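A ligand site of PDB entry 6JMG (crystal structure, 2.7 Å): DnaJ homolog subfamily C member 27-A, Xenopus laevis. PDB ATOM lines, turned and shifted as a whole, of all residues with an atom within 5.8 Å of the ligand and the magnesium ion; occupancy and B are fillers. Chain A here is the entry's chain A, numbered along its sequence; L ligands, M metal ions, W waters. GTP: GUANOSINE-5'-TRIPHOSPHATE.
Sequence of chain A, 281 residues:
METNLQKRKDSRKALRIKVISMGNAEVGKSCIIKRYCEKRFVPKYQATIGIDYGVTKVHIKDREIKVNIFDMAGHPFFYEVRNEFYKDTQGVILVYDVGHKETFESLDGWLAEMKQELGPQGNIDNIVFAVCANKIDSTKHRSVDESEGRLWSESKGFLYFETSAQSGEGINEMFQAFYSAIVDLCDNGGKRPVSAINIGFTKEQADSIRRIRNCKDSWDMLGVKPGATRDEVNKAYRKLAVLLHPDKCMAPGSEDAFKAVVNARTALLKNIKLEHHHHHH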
ATOM      1  N   GLY A  23      17.873  -4.414  13.632  1.00  0.00           N
ATOM      2  CA  GLY A  23      19.175  -3.805  13.449  1.00  0.00           C
ATOM      3  C   GLY A  23      19.628  -3.114  14.728  1.00  0.00           C
ATOM      4  O   GLY A  23      18.843  -2.836  15.644  1.00  0.00           O
ATOM      5  N   ASN A  24      20.922  -2.819  14.791  1.00  0.00           N
ATOM      6  CA  ASN A  24      21.543  -2.315  16.011  1.00  0.00           C
ATOM      7  C   ASN A  24      20.930  -0.980  16.443  1.00  0.00           C
ATOM      8  O   ASN A  24      20.197  -0.317  15.700  1.00  0.00           O
ATOM      9  CB  ASN A  24      23.049  -2.174  15.804  1.00  0.00           C
ATOM     10  CG  ASN A  24      23.777  -3.531  15.851  1.00  0.00           C
ATOM     11  OD1 ASN A  24      23.145  -4.582  15.903  1.00  0.00           O
ATOM     12  ND2 ASN A  24      25.099  -3.498  15.829  1.00  0.00           N
ATOM     13  N   ALA A  25      21.215  -0.599  17.690  1.00  0.00           N
ATOM     14  CA  ALA A  25      20.732   0.670  18.202  1.00  0.00           C
ATOM     15  C   ALA A  25      21.342   1.841  17.427  1.00  0.00           C
ATOM     16  O   ALA A  25      22.475   1.759  16.930  1.00  0.00           O
ATOM     17  CB  ALA A  25      21.057   0.803  19.684  1.00  0.00           C
ATOM     18  N   GLU A  26      20.579   2.940  17.336  1.00  0.00           N
ATOM     19  CA  GLU A  26      20.983   4.214  16.742  1.00  0.00           C
ATOM     20  C   GLU A  26      21.131   4.131  15.231  1.00  0.00           C
ATOM     21  O   GLU A  26      21.601   5.080  14.594  1.00  0.00           O
ATOM     22  CB  GLU A  26      22.307   4.734  17.331  1.00  0.00           C
ATOM     23  CG  GLU A  26      22.165   5.289  18.722  1.00  0.00           C
ATOM     24  CD  GLU A  26      23.155   6.400  18.983  1.00  0.00           C
ATOM     25  OE1 GLU A  26      23.233   7.340  18.151  1.00  0.00           O
ATOM     26  OE2 GLU A  26      23.861   6.308  20.014  1.00  0.00           O
ATOM     27  N   VAL A  27      20.737   3.010  14.641  1.00  0.00           N
ATOM     28  CA  VAL A  27      20.918   2.803  13.222  1.00  0.00           C
ATOM     29  C   VAL A  27      19.884   3.539  12.373  1.00  0.00           C
ATOM     30  O   VAL A  27      20.167   3.849  11.211  1.00  0.00           O
ATOM     31  CB  VAL A  27      20.926   1.264  13.064  1.00  0.00           C
ATOM     32  CG1 VAL A  27      20.479   0.841  11.740  1.00  0.00           C
ATOM     33  CG2 VAL A  27      22.319   0.732  13.333  1.00  0.00           C
ATOM     34  N   GLY A  28      18.723   3.883  12.924  1.00  0.00           N
ATOM     35  CA  GLY A  28      17.705   4.608  12.205  1.00  0.00           C
ATOM     36  C   GLY A  28      16.400   3.862  11.911  1.00  0.00           C
ATOM     37  O   GLY A  28      15.672   4.267  11.004  1.00  0.00           O
ATOM     38  N   LYS A  29      16.084   2.800  12.669  1.00  0.00           N
ATOM     39  CA  LYS A  29      14.899   2.021  12.354  1.00  0.00           C
ATOM     40  C   LYS A  29      13.640   2.843  12.567  1.00  0.00           C
ATOM     41  O   LYS A  29      12.787   2.941  11.688  1.00  0.00           O
ATOM     42  CB  LYS A  29      14.845   0.771  13.241  1.00  0.00           C
ATOM     43  CG  LYS A  29      16.038  -0.166  13.042  1.00  0.00           C
ATOM     44  CD  LYS A  29      15.913  -1.433  13.891  1.00  0.00           C
ATOM     45  CE  LYS A  29      16.127  -1.155  15.382  1.00  0.00           C
ATOM     46  NZ  LYS A  29      17.391  -0.439  15.677  1.00  0.00           N
ATOM     47  N   SER A  30      13.520   3.465  13.736  1.00  0.00           N
ATOM     48  CA  SER A  30      12.353   4.298  13.987  1.00  0.00           C
ATOM     49  C   SER A  30      12.238   5.427  12.975  1.00  0.00           C
ATOM     50  O   SER A  30      11.132   5.723  12.496  1.00  0.00           O
ATOM     51  CB  SER A  30      12.383   4.802  15.416  1.00  0.00           C
ATOM     52  OG  SER A  30      12.578   3.715  16.266  1.00  0.00           O
ATOM     53  N   CYS A  31      13.374   6.063  12.603  1.00  0.00           N
ATOM     54  CA  CYS A  31      13.260   7.252  11.780  1.00  0.00           C
ATOM     55  C   CYS A  31      13.006   6.917  10.320  1.00  0.00           C
ATOM     56  O   CYS A  31      12.307   7.674   9.635  1.00  0.00           O
ATOM     57  CB  CYS A  31      14.522   8.140  11.821  1.00  0.00           C
ATOM     58  SG  CYS A  31      15.034   8.895  13.367  1.00  0.00           S
ATOM     59  N   ILE A  32      13.443   5.760   9.837  1.00  0.00           N
ATOM     60  CA  ILE A  32      12.989   5.302   8.524  1.00  0.00           C
ATOM     61  C   ILE A  32      11.473   5.149   8.511  1.00  0.00           C
ATOM     62  O   ILE A  32      10.792   5.633   7.601  1.00  0.00           O
ATOM     63  CB  ILE A  32      13.694   3.992   8.130  1.00  0.00           C
ATOM     64  CG1 ILE A  32      15.159   4.248   7.761  1.00  0.00           C
ATOM     65  CG2 ILE A  32      12.972   3.366   6.964  1.00  0.00           C
ATOM     66  CD1 ILE A  32      15.938   2.974   7.586  1.00  0.00           C
ATOM     67  N   PHE A  41      10.831  13.989  10.606  1.00  0.00           N
ATOM     68  CA  PHE A  41      12.173  13.564  10.974  1.00  0.00           C
ATOM     69  C   PHE A  41      12.795  14.565  11.953  1.00  0.00           C
ATOM     70  O   PHE A  41      12.832  15.770  11.667  1.00  0.00           O
ATOM     71  CB  PHE A  41      13.097  13.432   9.761  1.00  0.00           C
ATOM     72  CG  PHE A  41      14.532  13.208  10.133  1.00  0.00           C
ATOM     73  CD1 PHE A  41      15.001  11.926  10.443  1.00  0.00           C
ATOM     74  CD2 PHE A  41      15.414  14.291  10.247  1.00  0.00           C
ATOM     75  CE1 PHE A  41      16.301  11.733  10.827  1.00  0.00           C
ATOM     76  CE2 PHE A  41      16.722  14.091  10.630  1.00  0.00           C
ATOM     77  CZ  PHE A  41      17.175  12.823  10.910  1.00  0.00           C
ATOM     78  N   VAL A  42      13.331  14.059  13.056  1.00  0.00           N
ATOM     79  CA  VAL A  42      14.044  14.893  14.017  1.00  0.00           C
ATOM     80  C   VAL A  42      15.431  14.311  14.267  1.00  0.00           C
ATOM     81  O   VAL A  42      15.595  13.085  14.271  1.00  0.00           O
ATOM     82  CB  VAL A  42      13.260  15.087  15.336  1.00  0.00           C
ATOM     83  CG1 VAL A  42      11.953  15.813  15.061  1.00  0.00           C
ATOM     84  CG2 VAL A  42      13.093  13.775  16.107  1.00  0.00           C
ATOM     85  N   PRO A  43      16.463  15.145  14.444  1.00  0.00           N
ATOM     86  CA  PRO A  43      17.793  14.605  14.734  1.00  0.00           C
ATOM     87  C   PRO A  43      17.946  14.058  16.153  1.00  0.00           C
ATOM     88  O   PRO A  43      18.879  13.300  16.415  1.00  0.00           O
ATOM     89  CB  PRO A  43      18.708  15.824  14.514  1.00  0.00           C
ATOM     90  CG  PRO A  43      17.813  17.005  14.783  1.00  0.00           C
ATOM     91  CD  PRO A  43      16.493  16.606  14.222  1.00  0.00           C
ATOM     92  N   LYS A  44      17.045  14.418  17.070  1.00  0.00           N
ATOM     93  CA  LYS A  44      17.186  14.019  18.457  1.00  0.00           C
ATOM     94  C   LYS A  44      16.830  12.547  18.624  1.00  0.00           C
ATOM     95  O   LYS A  44      15.760  12.109  18.200  1.00  0.00           O
ATOM     96  CB  LYS A  44      16.275  14.907  19.313  1.00  0.00           C
ATOM     97  CG  LYS A  44      16.286  14.648  20.789  1.00  0.00           C
ATOM     98  CD  LYS A  44      15.340  15.645  21.463  1.00  0.00           C
ATOM     99  CE  LYS A  44      15.508  15.610  22.982  1.00  0.00           C
ATOM    100  NZ  LYS A  44      16.948  15.464  23.372  1.00  0.00           N
ATOM    101  N   TYR A  45      17.733  11.787  19.246  1.00  0.00           N
ATOM    102  CA  TYR A  45      17.616  10.336  19.388  1.00  0.00           C
ATOM    103  C   TYR A  45      16.677   9.985  20.541  1.00  0.00           C
ATOM    104  O   TYR A  45      16.879  10.452  21.658  1.00  0.00           O
ATOM    105  CB  TYR A  45      18.990   9.725  19.619  1.00  0.00           C
ATOM    106  CG  TYR A  45      19.026   8.232  19.910  1.00  0.00           C
ATOM    107  CD1 TYR A  45      18.241   7.337  19.191  1.00  0.00           C
ATOM    108  CD2 TYR A  45      19.864   7.726  20.898  1.00  0.00           C
ATOM    109  CE1 TYR A  45      18.286   5.985  19.449  1.00  0.00           C
ATOM    110  CE2 TYR A  45      19.916   6.381  21.175  1.00  0.00           C
ATOM    111  CZ  TYR A  45      19.131   5.501  20.446  1.00  0.00           C
ATOM    112  OH  TYR A  45      19.197   4.157  20.723  1.00  0.00           O
ATOM    113  N   GLN A  46      15.635   9.197  20.264  1.00  0.00           N
ATOM    114  CA  GLN A  46      14.821   8.585  21.310  1.00  0.00           C
ATOM    115  C   GLN A  46      14.843   7.061  21.122  1.00  0.00           C
ATOM    116  O   GLN A  46      14.138   6.512  20.264  1.00  0.00           O
ATOM    117  CB  GLN A  46      13.404   9.137  21.321  1.00  0.00           C
ATOM    118  CG  GLN A  46      12.808   9.268  22.718  1.00  0.00           C
ATOM    119  CD  GLN A  46      13.766   9.940  23.729  1.00  0.00           C
ATOM    120  OE1 GLN A  46      14.345  11.006  23.447  1.00  0.00           O
ATOM    121  NE2 GLN A  46      13.946   9.304  24.890  1.00  0.00           N
ATOM    122  N   ALA A  47      15.669   6.366  21.913  1.00  0.00           N
ATOM    123  CA  ALA A  47      15.788   4.917  21.772  1.00  0.00           C
ATOM    124  C   ALA A  47      14.440   4.243  21.988  1.00  0.00           C
ATOM    125  O   ALA A  47      13.717   4.573  22.933  1.00  0.00           O
ATOM    126  CB  ALA A  47      16.805   4.352  22.758  1.00  0.00           C
ATOM    127  N   THR A  48      14.076   3.357  21.072  1.00  0.00           N
ATOM    128  CA  THR A  48      12.872   2.560  21.268  1.00  0.00           C
ATOM    129  C   THR A  48      13.046   1.699  22.504  1.00  0.00           C
ATOM    130  O   THR A  48      14.108   1.106  22.719  1.00  0.00           O
ATOM    131  CB  THR A  48      12.610   1.678  20.050  1.00  0.00           C
ATOM    132  OG1 THR A  48      12.530   2.522  18.883  1.00  0.00           O
ATOM    133  CG2 THR A  48      11.287   0.857  20.259  1.00  0.00           C
ATOM    134  N   ASP A  71       8.088  -1.920  15.556  1.00  0.00           N
ATOM    135  CA  ASP A  71       9.397  -1.302  15.462  1.00  0.00           C
ATOM    136  C   ASP A  71      10.188  -1.755  16.680  1.00  0.00           C
ATOM    137  O   ASP A  71       9.816  -1.446  17.810  1.00  0.00           O
ATOM    138  CB  ASP A  71       9.224   0.220  15.423  1.00  0.00           C
ATOM    139  CG  ASP A  71      10.533   0.969  15.506  1.00  0.00           C
ATOM    140  OD1 ASP A  71      11.599   0.395  15.222  1.00  0.00           O
ATOM    141  OD2 ASP A  71      10.496   2.157  15.872  1.00  0.00           O
ATOM    142  N   MET A  72      11.249  -2.556  16.450  1.00  0.00           N
ATOM    143  CA  MET A  72      11.951  -3.191  17.562  1.00  0.00           C
ATOM    144  C   MET A  72      13.115  -2.332  18.036  1.00  0.00           C
ATOM    145  O   MET A  72      13.738  -1.614  17.260  1.00  0.00           O
ATOM    146  CB  MET A  72      12.482  -4.583  17.193  1.00  0.00           C
ATOM    147  CG  MET A  72      11.483  -5.589  16.560  1.00  0.00           C
ATOM    148  SD  MET A  72      12.037  -7.335  16.508  1.00  0.00           S
ATOM    149  CE  MET A  72      13.593  -7.232  15.770  1.00  0.00           C
ATOM    150  N   ALA A  73      13.438  -2.480  19.314  1.00  0.00           N
ATOM    151  CA  ALA A  73      14.581  -1.817  19.902  1.00  0.00           C
ATOM    152  C   ALA A  73      15.838  -2.627  19.609  1.00  0.00           C
ATOM    153  O   ALA A  73      15.834  -3.856  19.695  1.00  0.00           O
ATOM    154  CB  ALA A  73      14.375  -1.679  21.413  1.00  0.00           C
ATOM    155  N   GLY A  74      16.908  -1.944  19.238  1.00  0.00           N
ATOM    156  CA  GLY A  74      18.089  -2.647  18.754  1.00  0.00           C
ATOM    157  C   GLY A  74      19.101  -3.025  19.826  1.00  0.00           C
ATOM    158  O   GLY A  74      19.972  -3.866  19.620  1.00  0.00           O
ATOM    159  N   HIS A  75      19.029  -2.353  20.963  1.00  0.00           N
ATOM    160  CA  HIS A  75      19.934  -2.657  22.056  1.00  0.00           C
ATOM    161  C   HIS A  75      19.759  -4.111  22.509  1.00  0.00           C
ATOM    162  O   HIS A  75      18.636  -4.603  22.597  1.00  0.00           O
ATOM    163  CB  HIS A  75      19.669  -1.693  23.210  1.00  0.00           C
ATOM    164  CG  HIS A  75      20.727  -1.717  24.264  1.00  0.00           C
ATOM    165  ND1 HIS A  75      20.880  -2.777  25.124  1.00  0.00           N
ATOM    166  CD2 HIS A  75      21.696  -0.832  24.580  1.00  0.00           C
ATOM    167  CE1 HIS A  75      21.891  -2.546  25.943  1.00  0.00           C
ATOM    168  NE2 HIS A  75      22.402  -1.362  25.630  1.00  0.00           N
ATOM    169  N   ASN A 134      21.638   2.748   5.729  1.00  0.00           N
ATOM    170  CA  ASN A 134      21.053   4.026   6.092  1.00  0.00           C
ATOM    171  C   ASN A 134      22.124   5.062   6.403  1.00  0.00           C
ATOM    172  O   ASN A 134      23.284   4.735   6.651  1.00  0.00           O
ATOM    173  CB  ASN A 134      20.137   3.874   7.290  1.00  0.00           C
ATOM    174  CG  ASN A 134      19.177   5.029   7.431  1.00  0.00           C
ATOM    175  OD1 ASN A 134      18.671   5.552   6.427  1.00  0.00           O
ATOM    176  ND2 ASN A 134      18.944   5.458   8.666  1.00  0.00           N
ATOM    177  N   LYS A 135      21.689   6.336   6.373  1.00  0.00           N
ATOM    178  CA  LYS A 135      22.501   7.507   6.726  1.00  0.00           C
ATOM    179  C   LYS A 135      23.564   7.815   5.662  1.00  0.00           C
ATOM    180  O   LYS A 135      24.636   8.329   5.984  1.00  0.00           O
ATOM    181  CB  LYS A 135      23.186   7.365   8.088  1.00  0.00           C
ATOM    182  CG  LYS A 135      22.269   6.964   9.222  1.00  0.00           C
ATOM    183  CD  LYS A 135      22.912   7.259  10.556  1.00  0.00           C
ATOM    184  CE  LYS A 135      21.977   6.957  11.687  1.00  0.00           C
ATOM    185  NZ  LYS A 135      22.702   6.842  12.968  1.00  0.00           N
ATOM    186  N   ILE A 136      23.240   7.553   4.392  1.00  0.00           N
ATOM    187  CA  ILE A 136      24.124   7.890   3.290  1.00  0.00           C
ATOM    188  C   ILE A 136      24.360   9.395   3.185  1.00  0.00           C
ATOM    189  O   ILE A 136      25.305   9.827   2.511  1.00  0.00           O
ATOM    190  CB  ILE A 136      23.560   7.329   1.961  1.00  0.00           C
ATOM    191  CG1 ILE A 136      22.140   7.832   1.713  1.00  0.00           C
ATOM    192  CG2 ILE A 136      23.570   5.822   1.972  1.00  0.00           C
ATOM    193  CD1 ILE A 136      21.555   7.264   0.414  1.00  0.00           C
ATOM    194  N   ASP A 137      23.511  10.203   3.812  1.00  0.00           N
ATOM    195  CA  ASP A 137      23.658  11.657   3.799  1.00  0.00           C
ATOM    196  C   ASP A 137      24.797  12.156   4.680  1.00  0.00           C
ATOM    197  O   ASP A 137      25.205  13.319   4.539  1.00  0.00           O
ATOM    198  CB  ASP A 137      22.366  12.300   4.296  1.00  0.00           C
ATOM    199  CG  ASP A 137      22.082  11.975   5.758  1.00  0.00           C
ATOM    200  OD1 ASP A 137      21.525  10.874   6.030  1.00  0.00           O
ATOM    201  OD2 ASP A 137      22.425  12.796   6.635  1.00  0.00           O
ATOM    202  N   SER A 138      25.317  11.341   5.590  1.00  0.00           N
ATOM    203  CA  SER A 138      26.244  11.878   6.564  1.00  0.00           C
ATOM    204  C   SER A 138      27.605  12.140   5.927  1.00  0.00           C
ATOM    205  O   SER A 138      28.067  11.386   5.065  1.00  0.00           O
ATOM    206  CB  SER A 138      26.384  10.937   7.752  1.00  0.00           C
ATOM    207  OG  SER A 138      27.677  11.073   8.309  1.00  0.00           O
ATOM    208  N   THR A 163      19.559   4.536   1.793  1.00  0.00           N
ATOM    209  CA  THR A 163      18.502   5.384   2.312  1.00  0.00           C
ATOM    210  C   THR A 163      19.094   6.426   3.241  1.00  0.00           C
ATOM    211  O   THR A 163      20.177   6.252   3.808  1.00  0.00           O
ATOM    212  CB  THR A 163      17.427   4.611   3.106  1.00  0.00           C
ATOM    213  OG1 THR A 163      18.033   3.902   4.192  1.00  0.00           O
ATOM    214  CG2 THR A 163      16.649   3.663   2.228  1.00  0.00           C
ATOM    215  N   SER A 164      18.315   7.481   3.401  1.00  0.00           N
ATOM    216  CA  SER A 164      18.543   8.472   4.437  1.00  0.00           C
ATOM    217  C   SER A 164      17.187   8.915   4.950  1.00  0.00           C
ATOM    218  O   SER A 164      16.379   9.470   4.201  1.00  0.00           O
ATOM    219  CB  SER A 164      19.333   9.688   3.929  1.00  0.00           C
ATOM    220  OG  SER A 164      19.309  10.761   4.867  1.00  0.00           O
ATOM    221  N   ALA A 165      16.954   8.673   6.239  1.00  0.00           N
ATOM    222  CA  ALA A 165      15.731   9.200   6.828  1.00  0.00           C
ATOM    223  C   ALA A 165      15.808  10.712   6.965  1.00  0.00           C
ATOM    224  O   ALA A 165      14.763  11.368   7.017  1.00  0.00           O
ATOM    225  CB  ALA A 165      15.483   8.548   8.196  1.00  0.00           C
ATOM    226  N   GLN A 166      17.023  11.274   7.013  1.00  0.00           N
ATOM    227  CA  GLN A 166      17.180  12.711   7.161  1.00  0.00           C
ATOM    228  C   GLN A 166      16.861  13.432   5.870  1.00  0.00           C
ATOM    229  O   GLN A 166      16.096  14.399   5.862  1.00  0.00           O
ATOM    230  CB  GLN A 166      18.600  13.025   7.622  1.00  0.00           C
ATOM    231  CG  GLN A 166      18.837  14.490   7.947  1.00  0.00           C
ATOM    232  CD  GLN A 166      19.311  15.265   6.743  1.00  0.00           C
ATOM    233  OE1 GLN A 166      20.013  14.724   5.883  1.00  0.00           O
ATOM    234  NE2 GLN A 166      18.910  16.531   6.653  1.00  0.00           N
ATOM    235  N   SER A 167      17.394  12.958   4.751  1.00  0.00           N
ATOM    236  CA  SER A 167      17.184  13.576   3.451  1.00  0.00           C
ATOM    237  C   SER A 167      15.936  13.063   2.732  1.00  0.00           C
ATOM    238  O   SER A 167      15.447  13.737   1.825  1.00  0.00           O
ATOM    239  CB  SER A 167      18.395  13.311   2.567  1.00  0.00           C
ATOM    240  OG  SER A 167      18.243  12.082   1.855  1.00  0.00           O
HETATM  241  PG  GTP L   1      16.866   2.167  18.582  1.00  0.00           P
HETATM  242  O1G GTP L   1      15.362   2.291  18.613  1.00  0.00           O
HETATM  243  O2G GTP L   1      17.305   0.765  18.234  1.00  0.00           O
HETATM  244  O3G GTP L   1      17.422   2.530  19.946  1.00  0.00           O
HETATM  245  O3B GTP L   1      17.555   3.084  17.441  1.00  0.00           O
HETATM  246  PB  GTP L   1      16.901   3.317  15.986  1.00  0.00           P
HETATM  247  O1B GTP L   1      17.376   2.285  15.000  1.00  0.00           O
HETATM  248  O2B GTP L   1      15.400   3.356  15.969  1.00  0.00           O
HETATM  249  O3A GTP L   1      17.559   4.715  15.546  1.00  0.00           O
HETATM  250  PA  GTP L   1      16.702   6.066  15.391  1.00  0.00           P
HETATM  251  O1A GTP L   1      15.661   5.976  14.299  1.00  0.00           O
HETATM  252  O2A GTP L   1      16.047   6.454  16.684  1.00  0.00           O
HETATM  253  O5' GTP L   1      17.883   7.071  15.031  1.00  0.00           O
HETATM  254  C5' GTP L   1      19.005   7.158  15.882  1.00  0.00           C
HETATM  255  C4' GTP L   1      19.633   8.524  15.683  1.00  0.00           C
HETATM  256  O4' GTP L   1      20.133   8.583  14.373  1.00  0.00           O
HETATM  257  C3' GTP L   1      18.659   9.678  15.794  1.00  0.00           C
HETATM  258  O3' GTP L   1      19.416  10.704  16.361  1.00  0.00           O
HETATM  259  C2' GTP L   1      18.333  10.099  14.380  1.00  0.00           C
HETATM  260  O2' GTP L   1      18.168  11.484  14.193  1.00  0.00           O
HETATM  261  C1' GTP L   1      19.586   9.691  13.658  1.00  0.00           C
HETATM  262  N9  GTP L   1      19.299   9.279  12.281  1.00  0.00           N
HETATM  263  C8  GTP L   1      18.409   8.317  11.875  1.00  0.00           C
HETATM  264  N7  GTP L   1      18.496   8.213  10.516  1.00  0.00           N
HETATM  265  C5  GTP L   1      19.431   9.089  10.072  1.00  0.00           C
HETATM  266  C6  GTP L   1      19.904   9.382   8.808  1.00  0.00           C
HETATM  267  O6  GTP L   1      19.459   8.817   7.817  1.00  0.00           O
HETATM  268  N1  GTP L   1      20.906  10.329   8.662  1.00  0.00           N
HETATM  269  C2  GTP L   1      21.414  10.975   9.751  1.00  0.00           C
HETATM  270  N2  GTP L   1      22.367  11.885   9.577  1.00  0.00           N
HETATM  271  N3  GTP L   1      20.941  10.683  11.025  1.00  0.00           N
HETATM  272  C4  GTP L   1      19.960   9.758  11.180  1.00  0.00           C
HETATM  273 MG    MG M   1      14.001   2.882  17.362  1.00  0.00          MG
HETATM  274  O   HOH W   1      14.270   4.893  18.065  1.00  0.00           O
HETATM  275  O   HOH W   2      17.733   0.387  21.596  1.00  0.00           O
HETATM  276  O   HOH W   3      13.607   0.958  16.578  1.00  0.00           O
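The backbone NH of Ser 30 is in hydrogen-bond range of an oxygen (O1A) of the ligand (3.3 Å).
N of Thr 48 lies close to O1G of the ligand, at 3.0 Å.
O3G of the ligand lies within hydrogen-bond range of OH of Tyr 45, at 2.5 Å.
The backbone carbonyl oxygen (O) of Pro 43 is in hydrogen-bond range of an oxygen (O3') of the ligand (2.7 Å).
The backbone NH (N) of Lys 29 sits at hydrogen-bond distance from an oxygen (O1B) of the ligand (2.7 Å).
The side-chain amino group (NZ) of Lys 29 is in salt-bridge range of an oxygen (O1B) of the ligand.
N1 of the ligand sits at hydrogen-bond distance from OD1 of Asp 137 (2.8 Å).
O1A of the ligand sits at hydrogen-bond distance from N of Cys 31 (2.8 Å).
The side-chain sulfur (SG) of Cys 31 is in hydrogen-bond range of an oxygen (O1A) of the ligand.
N of Gly 74 sits at hydrogen-bond distance from O2G of the ligand (2.9 Å).
O1B of the ligand sits at hydrogen-bond distance from N of Gly 28.
An oxygen (O6) of the ligand lies within hydrogen-bond range of the backbone NH (N) of Ala 165, 3.0 Å away.
N of Glu 26 is in hydrogen-bond range of O3B of the ligand.
The backbone carbonyl oxygen (O) of Val 42 sits at hydrogen-bond distance from an oxygen (O2') of the ligand.
A nitrogen (N7) of the ligand is in hydrogen-bond range of the side-chain amide nitrogen (ND2) of Asn 134.
An oxygen (O4') of the ligand is in hydrogen-bond range of the side-chain amino group of Lys 135 (3.4 Å).
The backbone NH of Val 27 is in hydrogen-bond range of an oxygen (O1B) of the ligand, at 3.5 Å.
The side-chain hydroxyl of Ser 30 sits close to the side-chain carboxylate of Asp 71, 2.6 Å away.
The backbone carbonyl oxygen (O) of Asn 24 sits at hydrogen-bond distance from the side-chain amino group (NZ) of Lys 29, 2.8 Å away.
The side-chain amino group of Lys 29 lies within hydrogen-bond range of the backbone carbonyl oxygen of Gly 23 (2.8 Å).
The side-chain carboxylate (OD2) of Asp 137 lies close to the side-chain amide oxygen (OE1) of Gln 166 (3.2 Å).
The backbone carbonyl oxygen (O) of Glu 26 lies within hydrogen-bond range of the side-chain amino group (NZ) of Lys 135 (2.6 Å).
The side-chain amide oxygen of Asn 134 is in hydrogen-bond range of the side-chain hydroxyl of Thr 163 (2.9 Å).
The backbone NH of Lys 135 lies within hydrogen-bond range of the backbone carbonyl oxygen of Thr 163, at 3.0 Å.
N of Gln 166 lies close to OG of Ser 164, at 3.2 Å.
Merely in contact with the ligand: Ala 47, Ala 25, Ser 164, Gln 166, Phe 41, Lys 44, Asn 24 and Ala 73.
Hydrophobic or aromatic side chains within 4 Å of the ligand: Phe 41, Tyr 45, Ala 47 and Ala 165.
23 residues have an atom within 4 Å of the ligand: Asn 24, Ala 25, Glu 26, Val 27, Gly 28, Lys 29, Ser 30, Cys 31, Phe 41, Val 42, Pro 43, Lys 44, Tyr 45, Ala 47, Thr 48, Ala 73, Gly 74, Asn 134, Lys 135, Asp 137, Ser 164, Ala 165 and Gln 166.
Asp 71 touches the magnesium ion (OD2 to MG, 3.9 Å).
Within 4 Å of the magnesium ion: Ser 30, Thr 48 and Asp 71.
Along chain A the residues within 4 Å of the magnesium ion span positions 30 to 71.
The nearest printed residue that does not touch the magnesium ion is Met 72 (4.5 Å).
The magnesium ion is bound by O1G of the ligand (1.9 Å), OG of Ser 30 (2.0 Å), O2B of the ligand (2.0 Å), water W3 (2.1 Å), OG1 of Thr 48 (2.1 Å) and water W1 (2.1 Å).
The magnesium ion has six donor atoms within binding distance.
Water W3 bridges the side-chain carboxylate of Asp 71 and the backbone carbonyl oxygen of Met 72.
Water W1 lies within hydrogen-bond range of O of Gln 46 (2.7 Å), O2A of the ligand (2.7 Å) and N of Thr 48 (3.4 Å).
Water W2 lies within hydrogen-bond range of O3G of the ligand, N of His 75 and N of Gly 74.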
